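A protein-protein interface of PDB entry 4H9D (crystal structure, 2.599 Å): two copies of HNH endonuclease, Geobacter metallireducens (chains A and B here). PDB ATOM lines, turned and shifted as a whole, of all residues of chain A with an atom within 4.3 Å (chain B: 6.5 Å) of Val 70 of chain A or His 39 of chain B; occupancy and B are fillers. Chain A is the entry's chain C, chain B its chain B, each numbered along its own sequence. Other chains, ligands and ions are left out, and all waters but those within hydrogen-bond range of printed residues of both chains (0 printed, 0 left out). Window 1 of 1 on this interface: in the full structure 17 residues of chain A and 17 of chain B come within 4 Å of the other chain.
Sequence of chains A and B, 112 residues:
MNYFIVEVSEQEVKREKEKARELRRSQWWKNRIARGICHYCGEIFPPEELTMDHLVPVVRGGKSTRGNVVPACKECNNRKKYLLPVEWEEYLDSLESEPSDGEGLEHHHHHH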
ATOM      1  N   TRP A  28     -25.073  -7.212 -30.256  1.00  0.00           N
ATOM      2  CA  TRP A  28     -24.186  -8.341 -30.020  1.00  0.00           C
ATOM      3  C   TRP A  28     -24.461  -9.456 -31.031  1.00  0.00           C
ATOM      4  O   TRP A  28     -23.536 -10.124 -31.500  1.00  0.00           O
ATOM      5  CB  TRP A  28     -24.345  -8.843 -28.578  1.00  0.00           C
ATOM      6  CG  TRP A  28     -24.936 -10.211 -28.423  1.00  0.00           C
ATOM      7  CD1 TRP A  28     -26.264 -10.541 -28.425  1.00  0.00           C
ATOM      8  CD2 TRP A  28     -24.216 -11.437 -28.217  1.00  0.00           C
ATOM      9  NE1 TRP A  28     -26.418 -11.898 -28.228  1.00  0.00           N
ATOM     10  CE2 TRP A  28     -25.179 -12.473 -28.099  1.00  0.00           C
ATOM     11  CE3 TRP A  28     -22.852 -11.764 -28.118  1.00  0.00           C
ATOM     12  CZ2 TRP A  28     -24.817 -13.818 -27.886  1.00  0.00           C
ATOM     13  CZ3 TRP A  28     -22.492 -13.100 -27.907  1.00  0.00           C
ATOM     14  CH2 TRP A  28     -23.475 -14.110 -27.793  1.00  0.00           C
ATOM     15  N   TRP A  29     -25.735  -9.621 -31.387  1.00  0.00           N
ATOM     16  CA  TRP A  29     -26.158 -10.646 -32.335  1.00  0.00           C
ATOM     17  C   TRP A  29     -26.034 -10.215 -33.794  1.00  0.00           C
ATOM     18  O   TRP A  29     -25.893 -11.051 -34.687  1.00  0.00           O
ATOM     19  CB  TRP A  29     -27.598 -11.058 -32.044  1.00  0.00           C
ATOM     20  CG  TRP A  29     -28.052 -12.218 -32.856  1.00  0.00           C
ATOM     21  CD1 TRP A  29     -28.818 -12.179 -33.981  1.00  0.00           C
ATOM     22  CD2 TRP A  29     -27.737 -13.596 -32.629  1.00  0.00           C
ATOM     23  NE1 TRP A  29     -29.002 -13.450 -34.472  1.00  0.00           N
ATOM     24  CE2 TRP A  29     -28.348 -14.339 -33.663  1.00  0.00           C
ATOM     25  CE3 TRP A  29     -26.997 -14.274 -31.654  1.00  0.00           C
ATOM     26  CZ2 TRP A  29     -28.242 -15.727 -33.751  1.00  0.00           C
ATOM     27  CZ3 TRP A  29     -26.892 -15.657 -31.740  1.00  0.00           C
ATOM     28  CH2 TRP A  29     -27.513 -16.369 -32.785  1.00  0.00           C
ATOM     29  N   ARG A  32     -22.604 -10.704 -34.510  1.00  0.00           N
ATOM     30  CA  ARG A  32     -22.448 -12.137 -34.369  1.00  0.00           C
ATOM     31  C   ARG A  32     -22.708 -12.830 -35.701  1.00  0.00           C
ATOM     32  O   ARG A  32     -21.808 -13.466 -36.262  1.00  0.00           O
ATOM     33  CB  ARG A  32     -23.423 -12.656 -33.319  1.00  0.00           C
ATOM     34  CG  ARG A  32     -22.928 -13.838 -32.514  1.00  0.00           C
ATOM     35  CD  ARG A  32     -21.920 -13.422 -31.458  1.00  0.00           C
ATOM     36  NE  ARG A  32     -21.817 -14.439 -30.417  1.00  0.00           N
ATOM     37  CZ  ARG A  32     -21.344 -15.663 -30.614  1.00  0.00           C
ATOM     38  NH1 ARG A  32     -20.913 -16.033 -31.812  1.00  0.00           N
ATOM     39  NH2 ARG A  32     -21.328 -16.531 -29.615  1.00  0.00           N
ATOM     40  N   HIS A  39     -21.265 -22.046 -34.309  1.00  0.00           N
ATOM     41  CA  HIS A  39     -20.648 -22.517 -33.071  1.00  0.00           C
ATOM     42  C   HIS A  39     -20.165 -23.954 -33.178  1.00  0.00           C
ATOM     43  O   HIS A  39     -19.024 -24.267 -32.834  1.00  0.00           O
ATOM     44  CB  HIS A  39     -21.649 -22.420 -31.913  1.00  0.00           C
ATOM     45  CG  HIS A  39     -21.142 -22.974 -30.613  1.00  0.00           C
ATOM     46  ND1 HIS A  39     -20.230 -22.310 -29.820  1.00  0.00           N
ATOM     47  CD2 HIS A  39     -21.439 -24.122 -29.961  1.00  0.00           C
ATOM     48  CE1 HIS A  39     -19.992 -23.023 -28.734  1.00  0.00           C
ATOM     49  NE2 HIS A  39     -20.713 -24.126 -28.796  1.00  0.00           N
ATOM     50  N   THR A  51     -28.741 -19.643 -38.144  1.00  0.00           N
ATOM     51  CA  THR A  51     -29.904 -19.642 -37.268  1.00  0.00           C
ATOM     52  C   THR A  51     -29.438 -19.359 -35.844  1.00  0.00           C
ATOM     53  O   THR A  51     -28.241 -19.406 -35.552  1.00  0.00           O
ATOM     54  CB  THR A  51     -30.577 -21.022 -37.250  1.00  0.00           C
ATOM     55  OG1 THR A  51     -30.466 -21.627 -38.547  1.00  0.00           O
ATOM     56  CG2 THR A  51     -32.053 -20.899 -36.854  1.00  0.00           C
ATOM     57  N   MET A  52     -30.382 -19.063 -34.962  1.00  0.00           N
ATOM     58  CA  MET A  52     -30.061 -18.826 -33.568  1.00  0.00           C
ATOM     59  C   MET A  52     -30.483 -20.078 -32.826  1.00  0.00           C
ATOM     60  O   MET A  52     -31.622 -20.525 -32.959  1.00  0.00           O
ATOM     61  CB  MET A  52     -30.840 -17.643 -33.015  1.00  0.00           C
ATOM     62  CG  MET A  52     -30.684 -17.507 -31.515  1.00  0.00           C
ATOM     63  SD  MET A  52     -31.865 -16.210 -30.716  1.00  0.00           S
ATOM     64  CE  MET A  52     -30.707 -14.653 -30.804  1.00  0.00           C
ATOM     65  N   ASP A  53     -29.573 -20.652 -32.051  1.00  0.00           N
ATOM     66  CA  ASP A  53     -29.892 -21.862 -31.302  1.00  0.00           C
ATOM     67  C   ASP A  53     -29.524 -21.682 -29.837  1.00  0.00           C
ATOM     68  O   ASP A  53     -28.588 -20.946 -29.503  1.00  0.00           O
ATOM     69  CB  ASP A  53     -29.142 -23.072 -31.886  1.00  0.00           C
ATOM     70  CG  ASP A  53     -29.607 -24.409 -31.291  1.00  0.00           C
ATOM     71  OD1 ASP A  53     -30.794 -24.773 -31.468  1.00  0.00           O
ATOM     72  OD2 ASP A  53     -28.780 -25.100 -30.650  1.00  0.00           O
ATOM     73  N   LEU A  55     -27.989 -23.218 -26.651  1.00  0.00           N
ATOM     74  CA  LEU A  55     -27.050 -24.253 -26.233  1.00  0.00           C
ATOM     75  C   LEU A  55     -27.758 -25.145 -25.218  1.00  0.00           C
ATOM     76  O   LEU A  55     -27.801 -26.369 -25.364  1.00  0.00           O
ATOM     77  CB  LEU A  55     -25.807 -23.590 -25.629  1.00  0.00           C
ATOM     78  CG  LEU A  55     -25.144 -22.562 -26.562  1.00  0.00           C
ATOM     79  CD1 LEU A  55     -24.124 -21.739 -25.809  1.00  0.00           C
ATOM     80  CD2 LEU A  55     -24.490 -23.270 -27.745  1.00  0.00           C
ATOM     81  N   ARG A  66     -27.496 -13.659 -23.924  1.00  0.00           N
ATOM     82  CA  ARG A  66     -26.173 -13.721 -24.547  1.00  0.00           C
ATOM     83  C   ARG A  66     -25.414 -15.030 -24.362  1.00  0.00           C
ATOM     84  O   ARG A  66     -24.847 -15.575 -25.310  1.00  0.00           O
ATOM     85  CB  ARG A  66     -25.284 -12.596 -24.027  1.00  0.00           C
ATOM     86  CG  ARG A  66     -25.366 -11.300 -24.797  1.00  0.00           C
ATOM     87  CD  ARG A  66     -24.019 -10.597 -24.747  1.00  0.00           C
ATOM     88  NE  ARG A  66     -24.046  -9.270 -25.352  1.00  0.00           N
ATOM     89  CZ  ARG A  66     -22.963  -8.625 -25.775  1.00  0.00           C
ATOM     90  NH1 ARG A  66     -21.769  -9.190 -25.658  1.00  0.00           N
ATOM     91  NH2 ARG A  66     -23.068  -7.415 -26.313  1.00  0.00           N
ATOM     92  N   GLY A  67     -25.393 -15.522 -23.131  1.00  0.00           N
ATOM     93  CA  GLY A  67     -24.673 -16.743 -22.840  1.00  0.00           C
ATOM     94  C   GLY A  67     -25.228 -17.999 -23.467  1.00  0.00           C
ATOM     95  O   GLY A  67     -24.494 -18.729 -24.129  1.00  0.00           O
ATOM     96  N   VAL A  69     -27.200 -18.522 -26.062  1.00  0.00           N
ATOM     97  CA  VAL A  69     -27.669 -18.404 -27.441  1.00  0.00           C
ATOM     98  C   VAL A  69     -26.493 -18.256 -28.396  1.00  0.00           C
ATOM     99  O   VAL A  69     -25.679 -17.346 -28.246  1.00  0.00           O
ATOM    100  CB  VAL A  69     -28.614 -17.196 -27.589  1.00  0.00           C
ATOM    101  CG1 VAL A  69     -28.682 -16.758 -29.029  1.00  0.00           C
ATOM    102  CG2 VAL A  69     -29.999 -17.568 -27.099  1.00  0.00           C
ATOM    103  N   VAL A  70     -26.424 -19.132 -29.395  1.00  0.00           N
ATOM    104  CA  VAL A  70     -25.315 -19.110 -30.343  1.00  0.00           C
ATOM    105  C   VAL A  70     -25.763 -19.283 -31.804  1.00  0.00           C
ATOM    106  O   VAL A  70     -26.850 -19.799 -32.069  1.00  0.00           O
ATOM    107  CB  VAL A  70     -24.311 -20.239 -29.965  1.00  0.00           C
ATOM    108  CG1 VAL A  70     -24.632 -21.507 -30.736  1.00  0.00           C
ATOM    109  CG2 VAL A  70     -22.883 -19.788 -30.182  1.00  0.00           C
ATOM    110  N   PRO A  71     -24.941 -18.817 -32.770  1.00  0.00           N
ATOM    111  CA  PRO A  71     -25.240 -18.931 -34.208  1.00  0.00           C
ATOM    112  C   PRO A  71     -25.031 -20.382 -34.625  1.00  0.00           C
ATOM    113  O   PRO A  71     -24.151 -21.060 -34.089  1.00  0.00           O
ATOM    114  CB  PRO A  71     -24.189 -18.036 -34.869  1.00  0.00           C
ATOM    115  CG  PRO A  71     -23.838 -17.061 -33.815  1.00  0.00           C
ATOM    116  CD  PRO A  71     -23.813 -17.891 -32.558  1.00  0.00           C
ATOM    117  N   ALA A  72     -25.817 -20.859 -35.581  1.00  0.00           N
ATOM    118  CA  ALA A  72     -25.676 -22.236 -36.047  1.00  0.00           C
ATOM    119  C   ALA A  72     -26.235 -22.363 -37.452  1.00  0.00           C
ATOM    120  O   ALA A  72     -27.355 -21.932 -37.714  1.00  0.00           O
ATOM    121  CB  ALA A  72     -26.407 -23.180 -35.108  1.00  0.00           C
ATOM    122  N   ARG B  32     -11.467 -22.685 -33.053  1.00  0.00           N
ATOM    123  CA  ARG B  32     -12.259 -21.833 -32.183  1.00  0.00           C
ATOM    124  C   ARG B  32     -11.375 -20.825 -31.436  1.00  0.00           C
ATOM    125  O   ARG B  32     -11.681 -19.623 -31.408  1.00  0.00           O
ATOM    126  CB  ARG B  32     -13.058 -22.699 -31.209  1.00  0.00           C
ATOM    127  CG  ARG B  32     -14.480 -22.209 -30.969  1.00  0.00           C
ATOM    128  CD  ARG B  32     -15.194 -21.851 -32.276  1.00  0.00           C
ATOM    129  NE  ARG B  32     -16.639 -21.715 -32.089  1.00  0.00           N
ATOM    130  CZ  ARG B  32     -17.220 -20.909 -31.203  1.00  0.00           C
ATOM    131  NH1 ARG B  32     -16.496 -20.145 -30.405  1.00  0.00           N
ATOM    132  NH2 ARG B  32     -18.537 -20.877 -31.103  1.00  0.00           N
ATOM    133  N   ILE B  37     -12.370 -15.069 -30.923  1.00  0.00           N
ATOM    134  CA  ILE B  37     -13.616 -14.427 -30.500  1.00  0.00           C
ATOM    135  C   ILE B  37     -14.213 -14.969 -29.195  1.00  0.00           C
ATOM    136  O   ILE B  37     -14.509 -16.159 -29.086  1.00  0.00           O
ATOM    137  CB  ILE B  37     -14.693 -14.570 -31.586  1.00  0.00           C
ATOM    138  CG1 ILE B  37     -14.064 -14.345 -32.965  1.00  0.00           C
ATOM    139  CG2 ILE B  37     -15.849 -13.597 -31.295  1.00  0.00           C
ATOM    140  CD1 ILE B  37     -15.022 -14.476 -34.101  1.00  0.00           C
ATOM    141  N   CYS B  38     -14.411 -14.088 -28.219  1.00  0.00           N
ATOM    142  CA  CYS B  38     -14.989 -14.487 -26.938  1.00  0.00           C
ATOM    143  C   CYS B  38     -16.503 -14.573 -27.029  1.00  0.00           C
ATOM    144  O   CYS B  38     -17.169 -13.588 -27.333  1.00  0.00           O
ATOM    145  CB  CYS B  38     -14.631 -13.486 -25.848  1.00  0.00           C
ATOM    146  SG  CYS B  38     -15.626 -13.687 -24.350  1.00  0.00           S
ATOM    147  N   HIS B  39     -17.045 -15.747 -26.731  1.00  0.00           N
ATOM    148  CA  HIS B  39     -18.478 -15.996 -26.791  1.00  0.00           C
ATOM    149  C   HIS B  39     -19.384 -14.906 -26.214  1.00  0.00           C
ATOM    150  O   HIS B  39     -20.363 -14.490 -26.840  1.00  0.00           O
ATOM    151  CB  HIS B  39     -18.772 -17.305 -26.065  1.00  0.00           C
ATOM    152  CG  HIS B  39     -20.227 -17.642 -25.988  1.00  0.00           C
ATOM    153  ND1 HIS B  39     -20.991 -17.902 -27.106  1.00  0.00           N
ATOM    154  CD2 HIS B  39     -21.044 -17.822 -24.924  1.00  0.00           C
ATOM    155  CE1 HIS B  39     -22.213 -18.234 -26.735  1.00  0.00           C
ATOM    156  NE2 HIS B  39     -22.272 -18.194 -25.416  1.00  0.00           N
ATOM    157  N   TYR B  40     -19.047 -14.470 -25.005  1.00  0.00           N
ATOM    158  CA  TYR B  40     -19.823 -13.489 -24.256  1.00  0.00           C
ATOM    159  C   TYR B  40     -19.799 -12.029 -24.713  1.00  0.00           C
ATOM    160  O   TYR B  40     -20.847 -11.463 -25.041  1.00  0.00           O
ATOM    161  CB  TYR B  40     -19.425 -13.580 -22.777  1.00  0.00           C
ATOM    162  CG  TYR B  40     -19.730 -14.936 -22.180  1.00  0.00           C
ATOM    163  CD1 TYR B  40     -21.050 -15.326 -21.927  1.00  0.00           C
ATOM    164  CD2 TYR B  40     -18.708 -15.867 -21.940  1.00  0.00           C
ATOM    165  CE1 TYR B  40     -21.351 -16.616 -21.458  1.00  0.00           C
ATOM    166  CE2 TYR B  40     -18.999 -17.156 -21.473  1.00  0.00           C
ATOM    167  CZ  TYR B  40     -20.325 -17.522 -21.242  1.00  0.00           C
ATOM    168  OH  TYR B  40     -20.629 -18.802 -20.846  1.00  0.00           O
ATOM    169  N   CYS B  41     -18.617 -11.422 -24.732  1.00  0.00           N
ATOM    170  CA  CYS B  41     -18.487 -10.016 -25.107  1.00  0.00           C
ATOM    171  C   CYS B  41     -18.104  -9.766 -26.562  1.00  0.00           C
ATOM    172  O   CYS B  41     -17.946  -8.623 -26.972  1.00  0.00           O
ATOM    173  CB  CYS B  41     -17.449  -9.358 -24.216  1.00  0.00           C
ATOM    174  SG  CYS B  41     -15.847 -10.037 -24.555  1.00  0.00           S
ATOM    175  N   GLY B  42     -17.922 -10.833 -27.328  1.00  0.00           N
ATOM    176  CA  GLY B  42     -17.576 -10.692 -28.734  1.00  0.00           C
ATOM    177  C   GLY B  42     -16.228 -10.104 -29.106  1.00  0.00           C
ATOM    178  O   GLY B  42     -15.939  -9.946 -30.286  1.00  0.00           O
ATOM    179  N   GLU B  43     -15.392  -9.779 -28.133  1.00  0.00           N
ATOM    180  CA  GLU B  43     -14.090  -9.213 -28.461  1.00  0.00           C
ATOM    181  C   GLU B  43     -13.099 -10.291 -28.907  1.00  0.00           C
ATOM    182  O   GLU B  43     -13.268 -11.480 -28.604  1.00  0.00           O
ATOM    183  CB  GLU B  43     -13.524  -8.446 -27.260  1.00  0.00           C
ATOM    184  CG  GLU B  43     -14.309  -7.177 -26.897  1.00  0.00           C
ATOM    185  CD  GLU B  43     -14.094  -6.029 -27.885  1.00  0.00           C
ATOM    186  OE1 GLU B  43     -14.140  -6.272 -29.112  1.00  0.00           O
ATOM    187  OE2 GLU B  43     -13.888  -4.879 -27.437  1.00  0.00           O
ATOM    188  N   LEU B  50      -8.031 -17.216 -24.032  1.00  0.00           N
ATOM    189  CA  LEU B  50      -9.411 -17.701 -24.045  1.00  0.00           C
ATOM    190  C   LEU B  50      -9.478 -19.021 -23.275  1.00  0.00           C
ATOM    191  O   LEU B  50      -8.590 -19.874 -23.394  1.00  0.00           O
ATOM    192  CB  LEU B  50      -9.895 -17.911 -25.482  1.00  0.00           C
ATOM    193  CG  LEU B  50      -9.832 -16.661 -26.366  1.00  0.00           C
ATOM    194  CD1 LEU B  50     -10.218 -17.044 -27.785  1.00  0.00           C
ATOM    195  CD2 LEU B  50     -10.755 -15.560 -25.822  1.00  0.00           C
ATOM    196  N   ASP B  53     -15.143 -22.618 -21.204  1.00  0.00           N
ATOM    197  CA  ASP B  53     -16.098 -22.379 -20.143  1.00  0.00           C
ATOM    198  C   ASP B  53     -17.344 -23.208 -20.385  1.00  0.00           C
ATOM    199  O   ASP B  53     -17.788 -23.342 -21.528  1.00  0.00           O
ATOM    200  CB  ASP B  53     -16.433 -20.888 -20.093  1.00  0.00           C
ATOM    201  CG  ASP B  53     -17.639 -20.590 -19.242  1.00  0.00           C
ATOM    202  OD1 ASP B  53     -17.617 -20.913 -18.033  1.00  0.00           O
ATOM    203  OD2 ASP B  53     -18.610 -20.026 -19.792  1.00  0.00           O
ATOM    204  N   LEU B  55     -21.377 -23.978 -19.926  1.00  0.00           N
ATOM    205  CA  LEU B  55     -22.622 -23.280 -19.659  1.00  0.00           C
ATOM    206  C   LEU B  55     -23.178 -23.912 -18.388  1.00  0.00           C
ATOM    207  O   LEU B  55     -23.167 -23.282 -17.330  1.00  0.00           O
ATOM    208  CB  LEU B  55     -23.583 -23.425 -20.834  1.00  0.00           C
ATOM    209  CG  LEU B  55     -23.609 -22.169 -21.713  1.00  0.00           C
ATOM    210  CD1 LEU B  55     -22.238 -21.871 -22.267  1.00  0.00           C
ATOM    211  CD2 LEU B  55     -24.596 -22.377 -22.832  1.00  0.00           C
ATOM    212  N   VAL B  70     -18.060 -23.282 -24.290  1.00  0.00           N
ATOM    213  CA  VAL B  70     -17.875 -22.153 -25.186  1.00  0.00           C
ATOM    214  C   VAL B  70     -16.612 -21.350 -24.867  1.00  0.00           C
ATOM    215  O   VAL B  70     -16.208 -21.257 -23.711  1.00  0.00           O
ATOM    216  CB  VAL B  70     -19.147 -21.250 -25.101  1.00  0.00           C
ATOM    217  CG1 VAL B  70     -19.034 -20.290 -23.939  1.00  0.00           C
ATOM    218  CG2 VAL B  70     -19.380 -20.536 -26.403  1.00  0.00           C
ATOM    219  N   PRO B  71     -15.972 -20.753 -25.889  1.00  0.00           N
ATOM    220  CA  PRO B  71     -14.745 -19.953 -25.705  1.00  0.00           C
ATOM    221  C   PRO B  71     -15.013 -18.665 -24.945  1.00  0.00           C
ATOM    222  O   PRO B  71     -15.917 -17.917 -25.297  1.00  0.00           O
ATOM    223  CB  PRO B  71     -14.302 -19.640 -27.126  1.00  0.00           C
ATOM    224  CG  PRO B  71     -15.054 -20.626 -27.981  1.00  0.00           C
ATOM    225  CD  PRO B  71     -16.363 -20.801 -27.305  1.00  0.00           C
ATOM    226  N   ALA B  72     -14.221 -18.391 -23.917  1.00  0.00           N
ATOM    227  CA  ALA B  72     -14.408 -17.179 -23.126  1.00  0.00           C
ATOM    228  C   ALA B  72     -13.077 -16.590 -22.706  1.00  0.00           C
ATOM    229  O   ALA B  72     -12.112 -17.325 -22.490  1.00  0.00           O
ATOM    230  CB  ALA B  72     -15.234 -17.479 -21.895  1.00  0.00           C
ATOM    231  N   CYS B  73     -13.024 -15.264 -22.592  1.00  0.00           N
ATOM    232  CA  CYS B  73     -11.798 -14.600 -22.176  1.00  0.00           C
ATOM    233  C   CYS B  73     -11.727 -14.650 -20.652  1.00  0.00           C
ATOM    234  O   CYS B  73     -12.734 -14.883 -19.986  1.00  0.00           O
ATOM    235  CB  CYS B  73     -11.783 -13.147 -22.666  1.00  0.00           C
ATOM    236  SG  CYS B  73     -13.040 -12.054 -21.940  1.00  0.00           S
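The backbone carbonyl oxygen of Tyr 40 of chain B sits at hydrogen-bond distance from the guanidinium group of Arg 66 of chain A. A ring nitrogen (NE2) of His 39 of chain B is in hydrogen-bond range of the backbone carbonyl oxygen of Gly 67 of chain A, at 2.6 Å. ND1 of His 39 of chain A lies within hydrogen-bond range of NH2 of Arg 32 of chain B (2.6 Å). NH2 of Arg 32 of chain A sits at hydrogen-bond distance from ND1 of His 39 of chain B.
The side-chain sulfur (SG) of Cys 41 of chain B lies close to the backbone NH (N) of Glu 43 of chain B (3.6 Å). N of Tyr 40 of chain B sits close to SG of Cys 38 of chain B (3.6 Å). O of Asp 53 of chain B sits at hydrogen-bond distance from N of Val 70 of chain B (2.8 Å). The backbone NH (N) of His 39 of chain A lies within hydrogen-bond range of the backbone carbonyl oxygen (O) of Pro 71 of chain A. O of Asp 53 of chain A sits at hydrogen-bond distance from N of Val 70 of chain A, at 2.8 Å. The side-chain hydroxyl of Tyr 40 of chain B is in hydrogen-bond range of the side-chain carboxylate of Asp 53 of chain B.
Of the 15 printed residues of chain B, 6 touch a printed residue of chain A. Hydrophobic or aromatic side chains of chain B that line the printed part of chain A: His 39, Tyr 40, Leu 55 and Val 70. Of the 14 printed residues of chain A, 8 touch a printed residue of chain B. Printed residues of chain A that touch a printed residue of chain B: Trp 28, Arg 32, His 39, Leu 55, Arg 66, Gly 67, Val 69 and Val 70. Hydrophobic or aromatic side chains of chain A that line the printed part of chain B: Trp 28, His 39, Leu 55 and Val 70. Among the printed residues, no Asp or Glu carboxylate lies within 4 Å of a Lys or Arg side-chain nitrogen of the other chain.
O of His 39 of chain B touches CZ3 of Trp 28 of chain A (2.8 Å). O of Tyr 40 of chain B touches CE3 of Trp 28 of chain A, 3.7 Å away. CE1 of His 39 of chain A touches CG2 of Val 70 of chain B, 3.5 Å away. Leu 55 of chain B touches Leu 55 of chain A. O of Arg 66 of chain A touches NE2 of His 39 of chain B, 3.7 Å away. Arg 66 of chain A touches Cys 41 of chain B. Tyr 40 of chain B touches Gly 67 of chain A (CE1 to CA, 3.6 Å). Leu 55 of chain B touches Gly 67 of chain A (CD2 to O, 3.9 Å). Val 69 of chain A touches His 39 of chain B (O to CE1, 3.9 Å). Val 70 of chain A touches His 39 of chain B (CG2 to CE1, 3.8 Å).
Printed residues of chain B within 4 Å of Trp 28 of chain A: His 39 (2.8 Å) and Tyr 40 (3.7 Å). Of the printed residues of chain B, Arg 32 of chain A touches His 39. Thr 51 of chain A touches none of the printed residues of chain B. Val 70 of chain A touches just one residue of chain B: His 39. Of the printed residues of chain A, His 39 of chain B touches Trp 28 (2.8 Å), Arg 32 (2.9 Å), Arg 66 (3.7 Å), Gly 67 (2.6 Å), Val 69 (3.9 Å) and Val 70 (3.8 Å). Printed residues of chain A within 4 Å of Val 70 of chain B: His 39 (3.5 Å). Pro 71 of chain B touches none of the printed residues of chain A. The nearest residue of chain B that does not touch Val 70 of chain A is Arg 32 of chain B (4.6 Å).
Arg 32 of chain A touches His 39 of chain B, and with the chains exchanged His 39 of chain A touches Arg 32 of chain B. His 39 of chain A touches Val 70 of chain B, and with the chains exchanged Val 70 of chain A touches His 39 of chain B. Leu 55 of chain B touches its own counterpart, Leu 55 of chain A. Of the 14 pairs that touch across the chains among the printed residues, 5 have their exchanged pair printed and touching as well.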
